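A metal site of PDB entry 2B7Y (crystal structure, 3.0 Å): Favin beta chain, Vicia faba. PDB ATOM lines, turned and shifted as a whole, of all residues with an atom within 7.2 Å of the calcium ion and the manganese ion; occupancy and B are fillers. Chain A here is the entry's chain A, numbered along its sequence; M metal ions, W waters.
The indole nitrogen (NE1) of Trp 129 lies close to the side-chain carboxylate (OD1) of Asp 130, at 3.2 Å. The backbone carbonyl oxygen of Glu 120 lies within hydrogen-bond range of the backbone NH of Gly 139 (2.7 Å). ND1 of His 137 is in hydrogen-bond range of O of Lys 135, 3.1 Å away.
Within 4 Å of the calcium ion: Asp 122, Phe 124, Asn 126 and Asp 130.
Along chain A the residues within 4 Å of the manganese ion span positions 120 to 137.
OD2 of Asp 130 binds the calcium ion (2.1 Å). OD2 of Asp 122 binds the calcium ion. The calcium ion is bound by O of Phe 124, at 2.3 Å. Water W4 is bound to the calcium ion, at 2.4 Å. The side-chain amide oxygen (OD1) of Asn 126 binds the calcium ion (2.4 Å). The calcium ion is bound by OD1 of Asp 122 (2.5 Å). Water W2 is bound to the calcium ion. The calcium ion has seven donor atoms within binding distance.
The manganese ion is bound by the side-chain carboxylate (OD1) of Asp 130 (2.0 Å), a ring nitrogen (NE2) of His 137 (2.2 Å), the side-chain carboxylate (OD2) of Asp 122 (2.4 Å) and water W1 (2.6 Å). The manganese ion has four donor atoms within binding distance. Slightly farther from the manganese ion lies OE1 of Glu 120 (2.8 Å). Slightly farther from the manganese ion lies water W3 (2.9 Å).
Water W2 bridges the backbone carbonyl oxygen (O) of Gly 100 and the indole nitrogen (NE1) of Trp 129. Water W1 bridges OG of Ser 147 (2.9 Å) and OE1 of Glu 120 (3.3 Å). Water W3 bridges the side-chain carboxylate (OE2) of Glu 120 and the indole nitrogen (NE1) of Trp 129.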
ATOM      1  N   ASP A  82      -7.543 -13.495  10.972  1.00  0.00           N
ATOM      2  CA  ASP A  82      -6.286 -14.206  10.989  1.00  0.00           C
ATOM      3  C   ASP A  82      -5.239 -13.175  10.586  1.00  0.00           C
ATOM      4  O   ASP A  82      -4.053 -13.263  10.958  1.00  0.00           O
ATOM      5  CB  ASP A  82      -6.374 -15.276   9.910  1.00  0.00           C
ATOM      6  CG  ASP A  82      -6.094 -16.654  10.427  1.00  0.00           C
ATOM      7  OD1 ASP A  82      -7.071 -17.409  10.707  1.00  0.00           O
ATOM      8  OD2 ASP A  82      -4.936 -17.049  10.583  1.00  0.00           O
ATOM      9  N   GLY A  83      -5.727 -12.192   9.802  1.00  0.00           N
ATOM     10  CA  GLY A  83      -4.982 -10.993   9.447  1.00  0.00           C
ATOM     11  C   GLY A  83      -5.278 -10.327   8.109  1.00  0.00           C
ATOM     12  O   GLY A  83      -6.185 -10.721   7.352  1.00  0.00           O
ATOM     13  N   GLY A  99      -7.159 -18.981   5.837  1.00  0.00           N
ATOM     14  CA  GLY A  99      -6.766 -18.833   7.258  1.00  0.00           C
ATOM     15  C   GLY A  99      -5.399 -18.222   7.463  1.00  0.00           C
ATOM     16  O   GLY A  99      -5.062 -17.161   6.919  1.00  0.00           O
ATOM     17  N   GLY A 100      -4.587 -18.915   8.250  1.00  0.00           N
ATOM     18  CA  GLY A 100      -3.184 -18.541   8.424  1.00  0.00           C
ATOM     19  C   GLY A 100      -2.408 -18.093   7.188  1.00  0.00           C
ATOM     20  O   GLY A 100      -1.476 -17.318   7.322  1.00  0.00           O
ATOM     21  N   TYR A 101      -2.752 -18.556   5.994  1.00  0.00           N
ATOM     22  CA  TYR A 101      -1.927 -18.139   4.857  1.00  0.00           C
ATOM     23  C   TYR A 101      -2.388 -16.794   4.203  1.00  0.00           C
ATOM     24  O   TYR A 101      -1.769 -16.309   3.215  1.00  0.00           O
ATOM     25  CB  TYR A 101      -1.781 -19.281   3.848  1.00  0.00           C
ATOM     26  CG  TYR A 101      -1.212 -20.570   4.454  1.00  0.00           C
ATOM     27  CD1 TYR A 101       0.178 -20.852   4.384  1.00  0.00           C
ATOM     28  CD2 TYR A 101      -2.051 -21.497   5.096  1.00  0.00           C
ATOM     29  CE1 TYR A 101       0.709 -22.040   4.935  1.00  0.00           C
ATOM     30  CE2 TYR A 101      -1.542 -22.660   5.640  1.00  0.00           C
ATOM     31  CZ  TYR A 101      -0.162 -22.943   5.569  1.00  0.00           C
ATOM     32  OH  TYR A 101       0.315 -24.113   6.155  1.00  0.00           O
ATOM     33  N   LEU A 102      -3.472 -16.210   4.765  1.00  0.00           N
ATOM     34  CA  LEU A 102      -4.031 -14.922   4.371  1.00  0.00           C
ATOM     35  C   LEU A 102      -4.378 -14.778   2.872  1.00  0.00           C
ATOM     36  O   LEU A 102      -4.354 -13.693   2.299  1.00  0.00           O
ATOM     37  CB  LEU A 102      -3.089 -13.811   4.844  1.00  0.00           C
ATOM     38  CG  LEU A 102      -2.548 -14.050   6.270  1.00  0.00           C
ATOM     39  CD1 LEU A 102      -1.313 -13.241   6.528  1.00  0.00           C
ATOM     40  CD2 LEU A 102      -3.562 -13.729   7.327  1.00  0.00           C
ATOM     41  N   GLU A 120       2.419  -8.135   6.135  1.00  0.00           N
ATOM     42  CA  GLU A 120       1.361  -8.816   6.850  1.00  0.00           C
ATOM     43  C   GLU A 120       1.153  -8.265   8.221  1.00  0.00           C
ATOM     44  O   GLU A 120       2.121  -8.087   8.996  1.00  0.00           O
ATOM     45  CB  GLU A 120       1.636 -10.328   6.954  1.00  0.00           C
ATOM     46  CG  GLU A 120       2.806 -10.732   7.847  1.00  0.00           C
ATOM     47  CD  GLU A 120       2.723 -12.180   8.323  1.00  0.00           C
ATOM     48  OE1 GLU A 120       3.764 -12.767   8.761  1.00  0.00           O
ATOM     49  OE2 GLU A 120       1.605 -12.750   8.260  1.00  0.00           O
ATOM     50  N   PHE A 121      -0.107  -8.001   8.538  1.00  0.00           N
ATOM     51  CA  PHE A 121      -0.478  -7.512   9.860  1.00  0.00           C
ATOM     52  C   PHE A 121      -1.193  -8.667  10.513  1.00  0.00           C
ATOM     53  O   PHE A 121      -2.400  -8.818  10.405  1.00  0.00           O
ATOM     54  CB  PHE A 121      -1.332  -6.240   9.753  1.00  0.00           C
ATOM     55  CG  PHE A 121      -0.655  -5.140   8.972  1.00  0.00           C
ATOM     56  CD1 PHE A 121      -0.533  -5.216   7.580  1.00  0.00           C
ATOM     57  CD2 PHE A 121      -0.075  -4.036   9.644  1.00  0.00           C
ATOM     58  CE1 PHE A 121       0.140  -4.203   6.862  1.00  0.00           C
ATOM     59  CE2 PHE A 121       0.587  -3.025   8.926  1.00  0.00           C
ATOM     60  CZ  PHE A 121       0.691  -3.114   7.514  1.00  0.00           C
ATOM     61  N   ASP A 122      -0.412  -9.495  11.168  1.00  0.00           N
ATOM     62  CA  ASP A 122      -0.857 -10.807  11.579  1.00  0.00           C
ATOM     63  C   ASP A 122      -1.538 -10.749  12.918  1.00  0.00           C
ATOM     64  O   ASP A 122      -0.945 -10.234  13.870  1.00  0.00           O
ATOM     65  CB  ASP A 122       0.358 -11.746  11.667  1.00  0.00           C
ATOM     66  CG  ASP A 122      -0.026 -13.197  11.743  1.00  0.00           C
ATOM     67  OD1 ASP A 122      -0.743 -13.576  12.691  1.00  0.00           O
ATOM     68  OD2 ASP A 122       0.364 -14.040  10.896  1.00  0.00           O
ATOM     69  N   THR A 123      -2.739 -11.281  13.020  1.00  0.00           N
ATOM     70  CA  THR A 123      -3.410 -11.195  14.317  1.00  0.00           C
ATOM     71  C   THR A 123      -3.736 -12.532  14.983  1.00  0.00           C
ATOM     72  O   THR A 123      -4.490 -12.557  15.964  1.00  0.00           O
ATOM     73  CB  THR A 123      -4.678 -10.345  14.245  1.00  0.00           C
ATOM     74  OG1 THR A 123      -5.666 -10.995  13.424  1.00  0.00           O
ATOM     75  CG2 THR A 123      -4.384  -9.060  13.524  1.00  0.00           C
ATOM     76  N   PHE A 124      -3.186 -13.631  14.446  1.00  0.00           N
ATOM     77  CA  PHE A 124      -3.418 -14.956  15.035  1.00  0.00           C
ATOM     78  C   PHE A 124      -2.182 -15.846  15.012  1.00  0.00           C
ATOM     79  O   PHE A 124      -1.616 -16.118  13.953  1.00  0.00           O
ATOM     80  CB  PHE A 124      -4.611 -15.665  14.379  1.00  0.00           C
ATOM     81  CG  PHE A 124      -4.953 -17.022  14.997  1.00  0.00           C
ATOM     82  CD1 PHE A 124      -4.217 -18.179  14.670  1.00  0.00           C
ATOM     83  CD2 PHE A 124      -6.043 -17.163  15.885  1.00  0.00           C
ATOM     84  CE1 PHE A 124      -4.546 -19.415  15.210  1.00  0.00           C
ATOM     85  CE2 PHE A 124      -6.373 -18.406  16.456  1.00  0.00           C
ATOM     86  CZ  PHE A 124      -5.629 -19.533  16.100  1.00  0.00           C
ATOM     87  N   TYR A 125      -1.808 -16.306  16.207  1.00  0.00           N
ATOM     88  CA  TYR A 125      -0.646 -17.165  16.404  1.00  0.00           C
ATOM     89  C   TYR A 125      -0.796 -18.556  15.749  1.00  0.00           C
ATOM     90  O   TYR A 125      -1.618 -19.388  16.109  1.00  0.00           O
ATOM     91  CB  TYR A 125      -0.292 -17.285  17.905  1.00  0.00           C
ATOM     92  CG  TYR A 125       0.890 -18.190  18.179  1.00  0.00           C
ATOM     93  CD1 TYR A 125       2.053 -18.041  17.426  1.00  0.00           C
ATOM     94  CD2 TYR A 125       0.854 -19.176  19.179  1.00  0.00           C
ATOM     95  CE1 TYR A 125       3.145 -18.828  17.644  1.00  0.00           C
ATOM     96  CE2 TYR A 125       1.959 -19.990  19.405  1.00  0.00           C
ATOM     97  CZ  TYR A 125       3.097 -19.782  18.629  1.00  0.00           C
ATOM     98  OH  TYR A 125       4.220 -20.525  18.745  1.00  0.00           O
ATOM     99  N   ASN A 126       0.016 -18.799  14.754  1.00  0.00           N
ATOM    100  CA  ASN A 126       0.033 -20.106  14.209  1.00  0.00           C
ATOM    101  C   ASN A 126       1.321 -20.776  14.700  1.00  0.00           C
ATOM    102  O   ASN A 126       2.436 -20.494  14.218  1.00  0.00           O
ATOM    103  CB  ASN A 126      -0.078 -20.001  12.708  1.00  0.00           C
ATOM    104  CG  ASN A 126      -1.361 -19.312  12.265  1.00  0.00           C
ATOM    105  OD1 ASN A 126      -1.305 -18.188  11.787  1.00  0.00           O
ATOM    106  ND2 ASN A 126      -2.511 -19.979  12.424  1.00  0.00           N
ATOM    107  N   ALA A 127       1.141 -21.639  15.719  1.00  0.00           N
ATOM    108  CA  ALA A 127       2.250 -22.183  16.501  1.00  0.00           C
ATOM    109  C   ALA A 127       3.295 -22.678  15.559  1.00  0.00           C
ATOM    110  O   ALA A 127       4.481 -22.602  15.821  1.00  0.00           O
ATOM    111  CB  ALA A 127       1.770 -23.316  17.414  1.00  0.00           C
ATOM    112  N   TRP A 129       4.309 -21.530  12.531  1.00  0.00           N
ATOM    113  CA  TRP A 129       5.293 -20.628  11.847  1.00  0.00           C
ATOM    114  C   TRP A 129       5.529 -19.218  12.336  1.00  0.00           C
ATOM    115  O   TRP A 129       6.566 -18.647  12.023  1.00  0.00           O
ATOM    116  CB  TRP A 129       4.955 -20.507  10.405  1.00  0.00           C
ATOM    117  CG  TRP A 129       3.672 -19.955  10.218  1.00  0.00           C
ATOM    118  CD1 TRP A 129       3.339 -18.639  10.264  1.00  0.00           C
ATOM    119  CD2 TRP A 129       2.501 -20.672   9.922  1.00  0.00           C
ATOM    120  NE1 TRP A 129       1.999 -18.499  10.021  1.00  0.00           N
ATOM    121  CE2 TRP A 129       1.459 -19.735   9.797  1.00  0.00           C
ATOM    122  CE3 TRP A 129       2.223 -22.024   9.729  1.00  0.00           C
ATOM    123  CZ2 TRP A 129       0.155 -20.122   9.495  1.00  0.00           C
ATOM    124  CZ3 TRP A 129       0.928 -22.408   9.442  1.00  0.00           C
ATOM    125  CH2 TRP A 129      -0.096 -21.460   9.323  1.00  0.00           C
ATOM    126  N   ASP A 130       4.532 -18.652  13.004  1.00  0.00           N
ATOM    127  CA  ASP A 130       4.611 -17.270  13.488  1.00  0.00           C
ATOM    128  C   ASP A 130       5.678 -17.158  14.598  1.00  0.00           C
ATOM    129  O   ASP A 130       6.159 -18.209  15.070  1.00  0.00           O
ATOM    130  CB  ASP A 130       3.223 -16.823  13.979  1.00  0.00           C
ATOM    131  CG  ASP A 130       2.245 -16.488  12.818  1.00  0.00           C
ATOM    132  OD1 ASP A 130       2.660 -15.936  11.756  1.00  0.00           O
ATOM    133  OD2 ASP A 130       1.029 -16.748  12.901  1.00  0.00           O
ATOM    134  N   PRO A 131       6.090 -15.948  15.008  1.00  0.00           N
ATOM    135  CA  PRO A 131       7.072 -15.842  16.033  1.00  0.00           C
ATOM    136  C   PRO A 131       6.434 -16.371  17.276  1.00  0.00           C
ATOM    137  O   PRO A 131       5.188 -16.364  17.420  1.00  0.00           O
ATOM    138  CB  PRO A 131       7.309 -14.343  16.153  1.00  0.00           C
ATOM    139  CG  PRO A 131       6.953 -13.830  14.896  1.00  0.00           C
ATOM    140  CD  PRO A 131       5.679 -14.608  14.562  1.00  0.00           C
ATOM    141  N   LYS A 135       2.915 -13.234  20.264  1.00  0.00           N
ATOM    142  CA  LYS A 135       2.351 -11.884  20.227  1.00  0.00           C
ATOM    143  C   LYS A 135       1.954 -11.571  18.787  1.00  0.00           C
ATOM    144  O   LYS A 135       2.649 -11.991  17.859  1.00  0.00           O
ATOM    145  CB  LYS A 135       3.395 -10.874  20.672  1.00  0.00           C
ATOM    146  CG  LYS A 135       3.641 -10.815  22.168  1.00  0.00           C
ATOM    147  CD  LYS A 135       3.771  -9.334  22.655  1.00  0.00           C
ATOM    148  CE  LYS A 135       3.932  -9.246  24.182  1.00  0.00           C
ATOM    149  NZ  LYS A 135       5.162 -10.013  24.624  1.00  0.00           N
ATOM    150  N   HIS A 137       1.794  -9.357  15.420  1.00  0.00           N
ATOM    151  CA  HIS A 137       2.965  -8.846  14.774  1.00  0.00           C
ATOM    152  C   HIS A 137       2.695  -8.398  13.335  1.00  0.00           C
ATOM    153  O   HIS A 137       1.700  -8.772  12.698  1.00  0.00           O
ATOM    154  CB  HIS A 137       4.011  -9.950  14.749  1.00  0.00           C
ATOM    155  CG  HIS A 137       3.526 -11.214  14.105  1.00  0.00           C
ATOM    156  ND1 HIS A 137       2.715 -12.118  14.774  1.00  0.00           N
ATOM    157  CD2 HIS A 137       3.712 -11.707  12.865  1.00  0.00           C
ATOM    158  CE1 HIS A 137       2.445 -13.124  13.972  1.00  0.00           C
ATOM    159  NE2 HIS A 137       3.038 -12.901  12.809  1.00  0.00           N
ATOM    160  N   ILE A 138       3.609  -7.587  12.820  1.00  0.00           N
ATOM    161  CA  ILE A 138       3.593  -7.277  11.410  1.00  0.00           C
ATOM    162  C   ILE A 138       4.838  -7.914  10.755  1.00  0.00           C
ATOM    163  O   ILE A 138       5.890  -8.117  11.397  1.00  0.00           O
ATOM    164  CB  ILE A 138       3.495  -5.769  11.197  1.00  0.00           C
ATOM    165  CG1 ILE A 138       4.825  -5.103  11.248  1.00  0.00           C
ATOM    166  CG2 ILE A 138       2.673  -5.061  12.282  1.00  0.00           C
ATOM    167  CD1 ILE A 138       4.610  -3.666  11.486  1.00  0.00           C
ATOM    168  N   GLY A 139       4.721  -8.298   9.503  1.00  0.00           N
ATOM    169  CA  GLY A 139       5.811  -9.044   8.934  1.00  0.00           C
ATOM    170  C   GLY A 139       6.009  -8.824   7.466  1.00  0.00           C
ATOM    171  O   GLY A 139       5.052  -8.615   6.720  1.00  0.00           O
ATOM    172  N   ASP A 141       6.847 -10.777   4.237  1.00  0.00           N
ATOM    173  CA  ASP A 141       6.785 -12.157   3.812  1.00  0.00           C
ATOM    174  C   ASP A 141       7.171 -12.144   2.391  1.00  0.00           C
ATOM    175  O   ASP A 141       6.788 -11.230   1.645  1.00  0.00           O
ATOM    176  CB  ASP A 141       5.355 -12.690   3.869  1.00  0.00           C
ATOM    177  CG  ASP A 141       4.756 -12.564   5.249  1.00  0.00           C
ATOM    178  OD1 ASP A 141       5.453 -12.087   6.189  1.00  0.00           O
ATOM    179  OD2 ASP A 141       3.586 -12.887   5.517  1.00  0.00           O
ATOM    180  N   ILE A 145       4.752 -17.831   4.144  1.00  0.00           N
ATOM    181  CA  ILE A 145       3.857 -17.232   5.103  1.00  0.00           C
ATOM    182  C   ILE A 145       4.637 -17.067   6.390  1.00  0.00           C
ATOM    183  O   ILE A 145       4.100 -16.662   7.413  1.00  0.00           O
ATOM    184  CB  ILE A 145       2.687 -18.141   5.323  1.00  0.00           C
ATOM    185  CG1 ILE A 145       1.551 -17.412   6.024  1.00  0.00           C
ATOM    186  CG2 ILE A 145       3.132 -19.333   6.167  1.00  0.00           C
ATOM    187  CD1 ILE A 145       1.241 -16.116   5.479  1.00  0.00           C
ATOM    188  N   LYS A 146       5.922 -17.401   6.323  1.00  0.00           N
ATOM    189  CA  LYS A 146       6.840 -17.325   7.459  1.00  0.00           C
ATOM    190  C   LYS A 146       7.765 -16.085   7.247  1.00  0.00           C
ATOM    191  O   LYS A 146       8.678 -16.116   6.407  1.00  0.00           O
ATOM    192  CB  LYS A 146       7.631 -18.627   7.489  1.00  0.00           C
ATOM    193  CG  LYS A 146       8.250 -18.963   8.783  1.00  0.00           C
ATOM    194  CD  LYS A 146       9.661 -19.472   8.548  1.00  0.00           C
ATOM    195  CE  LYS A 146      10.188 -20.172   9.780  1.00  0.00           C
ATOM    196  NZ  LYS A 146      11.493 -20.773   9.441  1.00  0.00           N
ATOM    197  N   SER A 147       7.488 -14.988   7.957  1.00  0.00           N
ATOM    198  CA  SER A 147       7.973 -13.655   7.523  1.00  0.00           C
ATOM    199  C   SER A 147       9.479 -13.599   7.675  1.00  0.00           C
ATOM    200  O   SER A 147      10.022 -14.125   8.651  1.00  0.00           O
ATOM    201  CB  SER A 147       7.335 -12.523   8.329  1.00  0.00           C
ATOM    202  OG  SER A 147       6.094 -12.909   8.912  1.00  0.00           O
ATOM    203  N   THR A 150       9.762  -9.630  11.599  1.00  0.00           N
ATOM    204  CA  THR A 150       8.559  -9.106  12.254  1.00  0.00           C
ATOM    205  C   THR A 150       8.874  -8.127  13.393  1.00  0.00           C
ATOM    206  O   THR A 150       9.973  -8.147  13.961  1.00  0.00           O
ATOM    207  CB  THR A 150       7.800 -10.224  12.895  1.00  0.00           C
ATOM    208  OG1 THR A 150       7.953 -10.096  14.317  1.00  0.00           O
ATOM    209  CG2 THR A 150       8.437 -11.604  12.560  1.00  0.00           C
HETATM  210 CA    CA M   1      -0.582 -15.887  11.885  1.00  0.00          CA
HETATM  211 MN    MN M   2       2.807 -14.067  11.000  1.00  0.00          MN
HETATM  212  O   HOH W   1       5.237 -14.930  10.806  1.00  0.00           O
HETATM  213  O   HOH W   2      -0.193 -16.583   9.455  1.00  0.00           O
HETATM  214  O   HOH W   3       2.519 -15.503   8.491  1.00  0.00           O
HETATM  215  O   HOH W   4      -2.861 -15.639  11.328  1.00  0.00           O
